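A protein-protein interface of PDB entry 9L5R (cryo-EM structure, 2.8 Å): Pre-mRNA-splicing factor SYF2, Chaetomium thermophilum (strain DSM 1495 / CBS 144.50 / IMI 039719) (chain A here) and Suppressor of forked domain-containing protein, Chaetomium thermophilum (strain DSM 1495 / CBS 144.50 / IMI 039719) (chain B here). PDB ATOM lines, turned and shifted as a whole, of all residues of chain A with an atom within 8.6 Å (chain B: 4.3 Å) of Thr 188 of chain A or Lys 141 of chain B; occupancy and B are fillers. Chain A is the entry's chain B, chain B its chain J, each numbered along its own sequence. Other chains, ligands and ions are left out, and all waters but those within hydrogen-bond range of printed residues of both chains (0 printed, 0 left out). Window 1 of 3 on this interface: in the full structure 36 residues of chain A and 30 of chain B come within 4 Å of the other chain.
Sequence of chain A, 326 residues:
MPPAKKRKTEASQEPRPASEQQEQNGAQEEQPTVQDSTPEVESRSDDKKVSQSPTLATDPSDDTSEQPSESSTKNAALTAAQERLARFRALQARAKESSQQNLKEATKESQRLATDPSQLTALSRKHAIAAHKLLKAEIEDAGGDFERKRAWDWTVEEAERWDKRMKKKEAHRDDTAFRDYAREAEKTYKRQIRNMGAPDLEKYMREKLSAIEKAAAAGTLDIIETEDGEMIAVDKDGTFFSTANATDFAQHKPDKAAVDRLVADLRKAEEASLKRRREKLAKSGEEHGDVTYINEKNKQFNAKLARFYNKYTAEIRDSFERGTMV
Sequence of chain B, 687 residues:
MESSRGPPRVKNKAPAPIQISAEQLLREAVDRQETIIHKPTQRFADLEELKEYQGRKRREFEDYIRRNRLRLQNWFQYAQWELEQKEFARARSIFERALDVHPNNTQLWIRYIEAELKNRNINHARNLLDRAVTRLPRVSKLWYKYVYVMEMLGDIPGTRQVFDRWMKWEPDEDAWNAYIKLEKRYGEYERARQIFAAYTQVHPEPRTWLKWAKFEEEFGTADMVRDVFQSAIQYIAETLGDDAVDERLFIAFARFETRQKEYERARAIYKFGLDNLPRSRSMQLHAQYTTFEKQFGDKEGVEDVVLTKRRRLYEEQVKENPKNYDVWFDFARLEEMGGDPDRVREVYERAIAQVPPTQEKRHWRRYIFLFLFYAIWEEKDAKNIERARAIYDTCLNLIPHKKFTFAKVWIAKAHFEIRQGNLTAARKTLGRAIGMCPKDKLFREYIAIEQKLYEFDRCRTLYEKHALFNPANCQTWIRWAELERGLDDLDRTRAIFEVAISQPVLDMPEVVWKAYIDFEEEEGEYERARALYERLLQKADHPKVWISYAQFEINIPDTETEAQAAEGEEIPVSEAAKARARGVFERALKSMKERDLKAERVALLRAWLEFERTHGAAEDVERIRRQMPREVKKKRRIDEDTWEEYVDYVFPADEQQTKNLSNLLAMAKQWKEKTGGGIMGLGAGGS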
ATOM      1  N   ASP A 175      28.968   3.120 -30.176  1.00  0.00           N
ATOM      2  CA  ASP A 175      28.222   2.468 -29.114  1.00  0.00           C
ATOM      3  C   ASP A 175      28.708   2.881 -27.729  1.00  0.00           C
ATOM      4  O   ASP A 175      28.320   2.264 -26.737  1.00  0.00           O
ATOM      5  CB  ASP A 175      28.329   0.955 -29.304  1.00  0.00           C
ATOM      6  CG  ASP A 175      27.208   0.187 -28.645  1.00  0.00           C
ATOM      7  OD1 ASP A 175      26.047   0.321 -29.083  1.00  0.00           O
ATOM      8  OD2 ASP A 175      27.500  -0.594 -27.727  1.00  0.00           O
ATOM      9  N   TYR A 181      20.208  -0.779 -20.644  1.00  0.00           N
ATOM     10  CA  TYR A 181      20.979  -1.714 -19.853  1.00  0.00           C
ATOM     11  C   TYR A 181      21.193  -3.033 -20.567  1.00  0.00           C
ATOM     12  O   TYR A 181      22.153  -3.727 -20.247  1.00  0.00           O
ATOM     13  CB  TYR A 181      20.321  -1.910 -18.497  1.00  0.00           C
ATOM     14  CG  TYR A 181      20.675  -0.799 -17.548  1.00  0.00           C
ATOM     15  CD1 TYR A 181      21.980  -0.615 -17.130  1.00  0.00           C
ATOM     16  CD2 TYR A 181      19.712   0.077 -17.087  1.00  0.00           C
ATOM     17  CE1 TYR A 181      22.314   0.394 -16.281  1.00  0.00           C
ATOM     18  CE2 TYR A 181      20.036   1.095 -16.238  1.00  0.00           C
ATOM     19  CZ  TYR A 181      21.341   1.246 -15.830  1.00  0.00           C
ATOM     20  OH  TYR A 181      21.689   2.254 -14.975  1.00  0.00           O
ATOM     21  N   ALA A 182      20.363  -3.371 -21.551  1.00  0.00           N
ATOM     22  CA  ALA A 182      20.635  -4.547 -22.368  1.00  0.00           C
ATOM     23  C   ALA A 182      21.903  -4.373 -23.194  1.00  0.00           C
ATOM     24  O   ALA A 182      22.715  -5.300 -23.290  1.00  0.00           O
ATOM     25  CB  ALA A 182      19.439  -4.847 -23.261  1.00  0.00           C
ATOM     26  N   ARG A 183      22.112  -3.184 -23.774  1.00  0.00           N
ATOM     27  CA  ARG A 183      23.371  -2.920 -24.467  1.00  0.00           C
ATOM     28  C   ARG A 183      24.544  -2.867 -23.515  1.00  0.00           C
ATOM     29  O   ARG A 183      25.625  -3.347 -23.855  1.00  0.00           O
ATOM     30  CB  ARG A 183      23.323  -1.629 -25.282  1.00  0.00           C
ATOM     31  CG  ARG A 183      22.354  -1.740 -26.343  1.00  0.00           C
ATOM     32  CD  ARG A 183      22.854  -2.732 -27.343  1.00  0.00           C
ATOM     33  NE  ARG A 183      21.946  -2.812 -28.471  1.00  0.00           N
ATOM     34  CZ  ARG A 183      20.935  -3.669 -28.502  1.00  0.00           C
ATOM     35  NH1 ARG A 183      20.642  -4.424 -27.452  1.00  0.00           N
ATOM     36  NH2 ARG A 183      20.178  -3.742 -29.593  1.00  0.00           N
ATOM     37  N   GLU A 184      24.367  -2.271 -22.338  1.00  0.00           N
ATOM     38  CA  GLU A 184      25.484  -2.232 -21.402  1.00  0.00           C
ATOM     39  C   GLU A 184      25.862  -3.630 -20.935  1.00  0.00           C
ATOM     40  O   GLU A 184      27.048  -3.940 -20.784  1.00  0.00           O
ATOM     41  CB  GLU A 184      25.159  -1.336 -20.216  1.00  0.00           C
ATOM     42  CG  GLU A 184      24.942   0.092 -20.587  1.00  0.00           C
ATOM     43  CD  GLU A 184      26.221   0.822 -20.931  1.00  0.00           C
ATOM     44  OE1 GLU A 184      27.233   0.628 -20.229  1.00  0.00           O
ATOM     45  OE2 GLU A 184      26.209   1.609 -21.900  1.00  0.00           O
ATOM     46  N   ALA A 185      24.870  -4.495 -20.731  1.00  0.00           N
ATOM     47  CA  ALA A 185      25.134  -5.867 -20.323  1.00  0.00           C
ATOM     48  C   ALA A 185      25.822  -6.660 -21.424  1.00  0.00           C
ATOM     49  O   ALA A 185      26.743  -7.432 -21.145  1.00  0.00           O
ATOM     50  CB  ALA A 185      23.833  -6.541 -19.907  1.00  0.00           C
ATOM     51  N   GLU A 186      25.403  -6.474 -22.677  1.00  0.00           N
ATOM     52  CA  GLU A 186      26.069  -7.148 -23.785  1.00  0.00           C
ATOM     53  C   GLU A 186      27.513  -6.676 -23.958  1.00  0.00           C
ATOM     54  O   GLU A 186      28.414  -7.496 -24.181  1.00  0.00           O
ATOM     55  CB  GLU A 186      25.276  -6.941 -25.068  1.00  0.00           C
ATOM     56  CG  GLU A 186      25.869  -7.638 -26.260  1.00  0.00           C
ATOM     57  CD  GLU A 186      25.273  -7.163 -27.566  1.00  0.00           C
ATOM     58  OE1 GLU A 186      24.474  -6.207 -27.547  1.00  0.00           O
ATOM     59  OE2 GLU A 186      25.595  -7.756 -28.617  1.00  0.00           O
ATOM     60  N   LYS A 187      27.755  -5.366 -23.833  1.00  0.00           N
ATOM     61  CA  LYS A 187      29.113  -4.838 -23.934  1.00  0.00           C
ATOM     62  C   LYS A 187      29.998  -5.358 -22.818  1.00  0.00           C
ATOM     63  O   LYS A 187      31.160  -5.714 -23.050  1.00  0.00           O
ATOM     64  CB  LYS A 187      29.105  -3.318 -23.877  1.00  0.00           C
ATOM     65  CG  LYS A 187      28.586  -2.608 -25.072  1.00  0.00           C
ATOM     66  CD  LYS A 187      28.063  -1.256 -24.649  1.00  0.00           C
ATOM     67  CE  LYS A 187      29.171  -0.367 -24.155  1.00  0.00           C
ATOM     68  NZ  LYS A 187      28.699   1.034 -23.977  1.00  0.00           N
ATOM     69  N   THR A 188      29.465  -5.398 -21.597  1.00  0.00           N
ATOM     70  CA  THR A 188      30.238  -5.864 -20.458  1.00  0.00           C
ATOM     71  C   THR A 188      30.572  -7.336 -20.590  1.00  0.00           C
ATOM     72  O   THR A 188      31.698  -7.744 -20.297  1.00  0.00           O
ATOM     73  CB  THR A 188      29.466  -5.588 -19.172  1.00  0.00           C
ATOM     74  OG1 THR A 188      29.160  -4.194 -19.103  1.00  0.00           O
ATOM     75  CG2 THR A 188      30.259  -5.974 -17.960  1.00  0.00           C
ATOM     76  N   TYR A 189      29.617  -8.143 -21.051  1.00  0.00           N
ATOM     77  CA  TYR A 189      29.884  -9.560 -21.232  1.00  0.00           C
ATOM     78  C   TYR A 189      30.936  -9.797 -22.305  1.00  0.00           C
ATOM     79  O   TYR A 189      31.843 -10.606 -22.105  1.00  0.00           O
ATOM     80  CB  TYR A 189      28.598 -10.305 -21.559  1.00  0.00           C
ATOM     81  CG  TYR A 189      28.801 -11.788 -21.725  1.00  0.00           C
ATOM     82  CD1 TYR A 189      29.079 -12.589 -20.636  1.00  0.00           C
ATOM     83  CD2 TYR A 189      28.716 -12.382 -22.973  1.00  0.00           C
ATOM     84  CE1 TYR A 189      29.269 -13.916 -20.782  1.00  0.00           C
ATOM     85  CE2 TYR A 189      28.899 -13.711 -23.126  1.00  0.00           C
ATOM     86  CZ  TYR A 189      29.175 -14.479 -22.029  1.00  0.00           C
ATOM     87  OH  TYR A 189      29.367 -15.827 -22.170  1.00  0.00           O
ATOM     88  N   LYS A 190      30.856  -9.082 -23.430  1.00  0.00           N
ATOM     89  CA  LYS A 190      31.846  -9.265 -24.491  1.00  0.00           C
ATOM     90  C   LYS A 190      33.241  -8.842 -24.048  1.00  0.00           C
ATOM     91  O   LYS A 190      34.234  -9.505 -24.375  1.00  0.00           O
ATOM     92  CB  LYS A 190      31.422  -8.500 -25.732  1.00  0.00           C
ATOM     93  CG  LYS A 190      30.418  -9.234 -26.564  1.00  0.00           C
ATOM     94  CD  LYS A 190      29.584  -8.279 -27.356  1.00  0.00           C
ATOM     95  CE  LYS A 190      29.258  -8.830 -28.706  1.00  0.00           C
ATOM     96  NZ  LYS A 190      28.279  -7.958 -29.378  1.00  0.00           N
ATOM     97  N   ARG A 191      33.334  -7.757 -23.285  1.00  0.00           N
ATOM     98  CA  ARG A 191      34.624  -7.329 -22.767  1.00  0.00           C
ATOM     99  C   ARG A 191      35.183  -8.330 -21.766  1.00  0.00           C
ATOM    100  O   ARG A 191      36.385  -8.600 -21.764  1.00  0.00           O
ATOM    101  CB  ARG A 191      34.481  -5.941 -22.151  1.00  0.00           C
ATOM    102  CG  ARG A 191      35.666  -5.433 -21.381  1.00  0.00           C
ATOM    103  CD  ARG A 191      35.262  -4.241 -20.552  1.00  0.00           C
ATOM    104  NE  ARG A 191      34.362  -3.354 -21.284  1.00  0.00           N
ATOM    105  CZ  ARG A 191      33.208  -2.893 -20.816  1.00  0.00           C
ATOM    106  NH1 ARG A 191      32.766  -3.225 -19.615  1.00  0.00           N
ATOM    107  NH2 ARG A 191      32.485  -2.069 -21.570  1.00  0.00           N
ATOM    108  N   GLN A 192      34.328  -8.914 -20.926  1.00  0.00           N
ATOM    109  CA  GLN A 192      34.787  -9.907 -19.960  1.00  0.00           C
ATOM    110  C   GLN A 192      35.254 -11.192 -20.636  1.00  0.00           C
ATOM    111  O   GLN A 192      36.213 -11.827 -20.178  1.00  0.00           O
ATOM    112  CB  GLN A 192      33.674 -10.206 -18.965  1.00  0.00           C
ATOM    113  CG  GLN A 192      33.476  -9.132 -17.946  1.00  0.00           C
ATOM    114  CD  GLN A 192      32.236  -9.335 -17.125  1.00  0.00           C
ATOM    115  OE1 GLN A 192      31.213  -9.792 -17.618  1.00  0.00           O
ATOM    116  NE2 GLN A 192      32.325  -9.011 -15.855  1.00  0.00           N
ATOM    117  N   ILE A 193      34.585 -11.598 -21.717  1.00  0.00           N
ATOM    118  CA  ILE A 193      35.053 -12.745 -22.492  1.00  0.00           C
ATOM    119  C   ILE A 193      36.425 -12.459 -23.096  1.00  0.00           C
ATOM    120  O   ILE A 193      37.330 -13.305 -23.045  1.00  0.00           O
ATOM    121  CB  ILE A 193      34.037 -13.121 -23.585  1.00  0.00           C
ATOM    122  CG1 ILE A 193      32.669 -13.479 -23.003  1.00  0.00           C
ATOM    123  CG2 ILE A 193      34.542 -14.268 -24.388  1.00  0.00           C
ATOM    124  CD1 ILE A 193      32.639 -14.582 -22.043  1.00  0.00           C
ATOM    125  N   ARG A 194      36.604 -11.261 -23.670  1.00  0.00           N
ATOM    126  CA  ARG A 194      37.912 -10.884 -24.202  1.00  0.00           C
ATOM    127  C   ARG A 194      38.977 -10.890 -23.115  1.00  0.00           C
ATOM    128  O   ARG A 194      40.117 -11.293 -23.355  1.00  0.00           O
ATOM    129  CB  ARG A 194      37.855  -9.507 -24.859  1.00  0.00           C
ATOM    130  CG  ARG A 194      37.042  -9.432 -26.127  1.00  0.00           C
ATOM    131  CD  ARG A 194      37.246  -8.106 -26.856  1.00  0.00           C
ATOM    132  NE  ARG A 194      36.878  -6.934 -26.068  1.00  0.00           N
ATOM    133  CZ  ARG A 194      35.757  -6.241 -26.220  1.00  0.00           C
ATOM    134  NH1 ARG A 194      34.835  -6.598 -27.095  1.00  0.00           N
ATOM    135  NH2 ARG A 194      35.558  -5.159 -25.478  1.00  0.00           N
ATOM    136  N   ASN A 195      38.621 -10.452 -21.910  1.00  0.00           N
ATOM    137  CA  ASN A 195      39.607 -10.376 -20.843  1.00  0.00           C
ATOM    138  C   ASN A 195      39.963 -11.743 -20.283  1.00  0.00           C
ATOM    139  O   ASN A 195      41.055 -11.906 -19.737  1.00  0.00           O
ATOM    140  CB  ASN A 195      39.118  -9.457 -19.732  1.00  0.00           C
ATOM    141  CG  ASN A 195      39.018  -8.032 -20.177  1.00  0.00           C
ATOM    142  OD1 ASN A 195      39.527  -7.670 -21.233  1.00  0.00           O
ATOM    143  ND2 ASN A 195      38.356  -7.207 -19.382  1.00  0.00           N
ATOM    144  N   ILE B 110      22.590  -7.661  -7.993  1.00  0.00           N
ATOM    145  CA  ILE B 110      24.000  -7.766  -8.348  1.00  0.00           C
ATOM    146  C   ILE B 110      24.893  -7.541  -7.132  1.00  0.00           C
ATOM    147  O   ILE B 110      25.880  -8.255  -6.952  1.00  0.00           O
ATOM    148  CB  ILE B 110      24.333  -6.800  -9.500  1.00  0.00           C
ATOM    149  CG1 ILE B 110      23.900  -7.402 -10.823  1.00  0.00           C
ATOM    150  CG2 ILE B 110      25.804  -6.544  -9.608  1.00  0.00           C
ATOM    151  CD1 ILE B 110      23.772  -6.402 -11.889  1.00  0.00           C
ATOM    152  N   VAL B 139      15.691  -9.751 -17.703  1.00  0.00           N
ATOM    153  CA  VAL B 139      16.834  -8.843 -17.436  1.00  0.00           C
ATOM    154  C   VAL B 139      18.077  -9.622 -17.839  1.00  0.00           C
ATOM    155  O   VAL B 139      18.476 -10.492 -17.094  1.00  0.00           O
ATOM    156  CB  VAL B 139      16.858  -8.333 -15.991  1.00  0.00           C
ATOM    157  CG1 VAL B 139      18.055  -7.442 -15.731  1.00  0.00           C
ATOM    158  CG2 VAL B 139      15.576  -7.602 -15.647  1.00  0.00           C
ATOM    159  N   SER B 140      18.615  -9.360 -19.004  1.00  0.00           N
ATOM    160  CA  SER B 140      19.748 -10.026 -19.608  1.00  0.00           C
ATOM    161  C   SER B 140      21.032  -9.773 -18.847  1.00  0.00           C
ATOM    162  O   SER B 140      21.950 -10.570 -18.963  1.00  0.00           O
ATOM    163  CB  SER B 140      19.893  -9.593 -21.059  1.00  0.00           C
ATOM    164  OG  SER B 140      20.358  -8.268 -21.139  1.00  0.00           O
ATOM    165  N   LYS B 141      21.102  -8.713 -18.042  1.00  0.00           N
ATOM    166  CA  LYS B 141      22.256  -8.514 -17.173  1.00  0.00           C
ATOM    167  C   LYS B 141      22.443  -9.671 -16.200  1.00  0.00           C
ATOM    168  O   LYS B 141      23.561 -10.160 -16.019  1.00  0.00           O
ATOM    169  CB  LYS B 141      22.114  -7.210 -16.406  1.00  0.00           C
ATOM    170  CG  LYS B 141      23.262  -6.933 -15.477  1.00  0.00           C
ATOM    171  CD  LYS B 141      24.476  -6.543 -16.234  1.00  0.00           C
ATOM    172  CE  LYS B 141      25.688  -6.511 -15.364  1.00  0.00           C
ATOM    173  NZ  LYS B 141      26.793  -5.861 -16.087  1.00  0.00           N
ATOM    174  N   LEU B 142      21.364 -10.125 -15.574  1.00  0.00           N
ATOM    175  CA  LEU B 142      21.489 -11.219 -14.628  1.00  0.00           C
ATOM    176  C   LEU B 142      21.817 -12.515 -15.341  1.00  0.00           C
ATOM    177  O   LEU B 142      22.628 -13.312 -14.852  1.00  0.00           O
ATOM    178  CB  LEU B 142      20.216 -11.352 -13.808  1.00  0.00           C
ATOM    179  CG  LEU B 142      19.892 -10.090 -13.020  1.00  0.00           C
ATOM    180  CD1 LEU B 142      18.466 -10.112 -12.601  1.00  0.00           C
ATOM    181  CD2 LEU B 142      20.808  -9.962 -11.834  1.00  0.00           C
ATOM    182  N   TRP B 143      21.230 -12.723 -16.519  1.00  0.00           N
ATOM    183  CA  TRP B 143      21.620 -13.914 -17.275  1.00  0.00           C
ATOM    184  C   TRP B 143      23.096 -13.888 -17.705  1.00  0.00           C
ATOM    185  O   TRP B 143      23.787 -14.914 -17.632  1.00  0.00           O
ATOM    186  CB  TRP B 143      20.716 -14.074 -18.478  1.00  0.00           C
ATOM    187  CG  TRP B 143      19.336 -14.571 -18.200  1.00  0.00           C
ATOM    188  CD1 TRP B 143      18.193 -13.860 -18.290  1.00  0.00           C
ATOM    189  CD2 TRP B 143      18.956 -15.894 -17.843  1.00  0.00           C
ATOM    190  NE1 TRP B 143      17.127 -14.637 -17.988  1.00  0.00           N
ATOM    191  CE2 TRP B 143      17.564 -15.899 -17.711  1.00  0.00           C
ATOM    192  CE3 TRP B 143      19.657 -17.075 -17.597  1.00  0.00           C
ATOM    193  CZ2 TRP B 143      16.851 -17.042 -17.351  1.00  0.00           C
ATOM    194  CZ3 TRP B 143      18.949 -18.202 -17.246  1.00  0.00           C
ATOM    195  CH2 TRP B 143      17.566 -18.178 -17.129  1.00  0.00           C
ATOM    196  N   TYR B 144      23.598 -12.727 -18.146  1.00  0.00           N
ATOM    197  CA  TYR B 144      24.995 -12.597 -18.552  1.00  0.00           C
ATOM    198  C   TYR B 144      25.942 -12.783 -17.382  1.00  0.00           C
ATOM    199  O   TYR B 144      27.006 -13.385 -17.532  1.00  0.00           O
ATOM    200  CB  TYR B 144      25.253 -11.229 -19.178  1.00  0.00           C
ATOM    201  CG  TYR B 144      24.896 -11.092 -20.628  1.00  0.00           C
ATOM    202  CD1 TYR B 144      25.371 -11.975 -21.566  1.00  0.00           C
ATOM    203  CD2 TYR B 144      24.106 -10.048 -21.059  1.00  0.00           C
ATOM    204  CE1 TYR B 144      25.057 -11.830 -22.881  1.00  0.00           C
ATOM    205  CE2 TYR B 144      23.778  -9.904 -22.363  1.00  0.00           C
ATOM    206  CZ  TYR B 144      24.262 -10.793 -23.270  1.00  0.00           C
ATOM    207  OH  TYR B 144      23.953 -10.655 -24.582  1.00  0.00           O
ATOM    208  N   LYS B 145      25.581 -12.253 -16.215  1.00  0.00           N
ATOM    209  CA  LYS B 145      26.386 -12.457 -15.023  1.00  0.00           C
ATOM    210  C   LYS B 145      26.455 -13.925 -14.652  1.00  0.00           C
ATOM    211  O   LYS B 145      27.513 -14.421 -14.267  1.00  0.00           O
ATOM    212  CB  LYS B 145      25.824 -11.646 -13.862  1.00  0.00           C
ATOM    213  CG  LYS B 145      26.641 -11.757 -12.603  1.00  0.00           C
ATOM    214  CD  LYS B 145      26.333 -10.676 -11.632  1.00  0.00           C
ATOM    215  CE  LYS B 145      27.482 -10.504 -10.672  1.00  0.00           C
ATOM    216  NZ  LYS B 145      28.771 -10.480 -11.402  1.00  0.00           N
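O of Glu 184 of chain A lies within hydrogen-bond range of OG1 of Thr 188 of chain A, at 2.7 Å.
The side-chain amino group of Lys 190 of chain A lies within salt-bridge range of the side-chain carboxylate of Glu 186 of chain A.
O of Thr 188 of chain A lies close to OE1 of Gln 192 of chain A (3.4 Å).
Hydrophobic or aromatic side chains of chain A that line the printed part of chain B: Ala 185 and Tyr 189.
Printed residues of chain B that touch a printed residue of chain A: Ser 140, Lys 141 and Tyr 144.
Hydrophobic or aromatic side chains of chain B within 4 Å of the printed part of chain A: Tyr 144.
Among the printed residues, 6 pairs touch across the chains.
Among the printed residues, no Asp or Glu carboxylate lies within 4 Å of a Lys or Arg side-chain nitrogen of the other chain.
CA of Ala 182 of chain A touches OG of Ser 140 of chain B, 3.9 Å away.
Ala 185 of chain A touches Lys 141 of chain B.
Ala 185 of chain A touches Tyr 144 of chain B.
N of Glu 186 of chain A touches CE2 of Tyr 144 of chain B, at 3.8 Å.
Thr 188 of chain A touches Lys 141 of chain B (CG2 to NZ, 3.9 Å).
Tyr 144 of chain B touches Tyr 189 of chain A (CD1 to CG, 3.4 Å).
Of the printed residues of chain B, Ala 182 of chain A touches Ser 140.
Of the printed residues of chain B, Ala 185 of chain A touches Lys 141 and Tyr 144.
Printed residues of chain B within 4 Å of Glu 186 of chain A: Tyr 144 (3.8 Å).
Thr 188 of chain A touches one residue of chain B.
Val 139 of chain B touches none of the printed residues of chain A.
Ser 140 of chain B touches just one residue of chain A: Ala 182 (3.9 Å).
Of chain A, only Ala 185 and Thr 188 come within 4 Å of Lys 141 of chain B.
Of the printed residues of chain A, Tyr 144 of chain B touches Ala 185 (3.7 Å), Glu 186 (3.8 Å) and Tyr 189 (3.4 Å).
The nearest printed residue of chain B that does not touch Thr 188 of chain A is Tyr 144 of chain B (6.7 Å).
The nearest residue of chain A that does not touch Lys 141 of chain B is Glu 184 of chain A (5.1 Å).
The nearest printed residue of chain B that does not touch Glu 186 of chain A is Ser 140 of chain B (5.6 Å).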
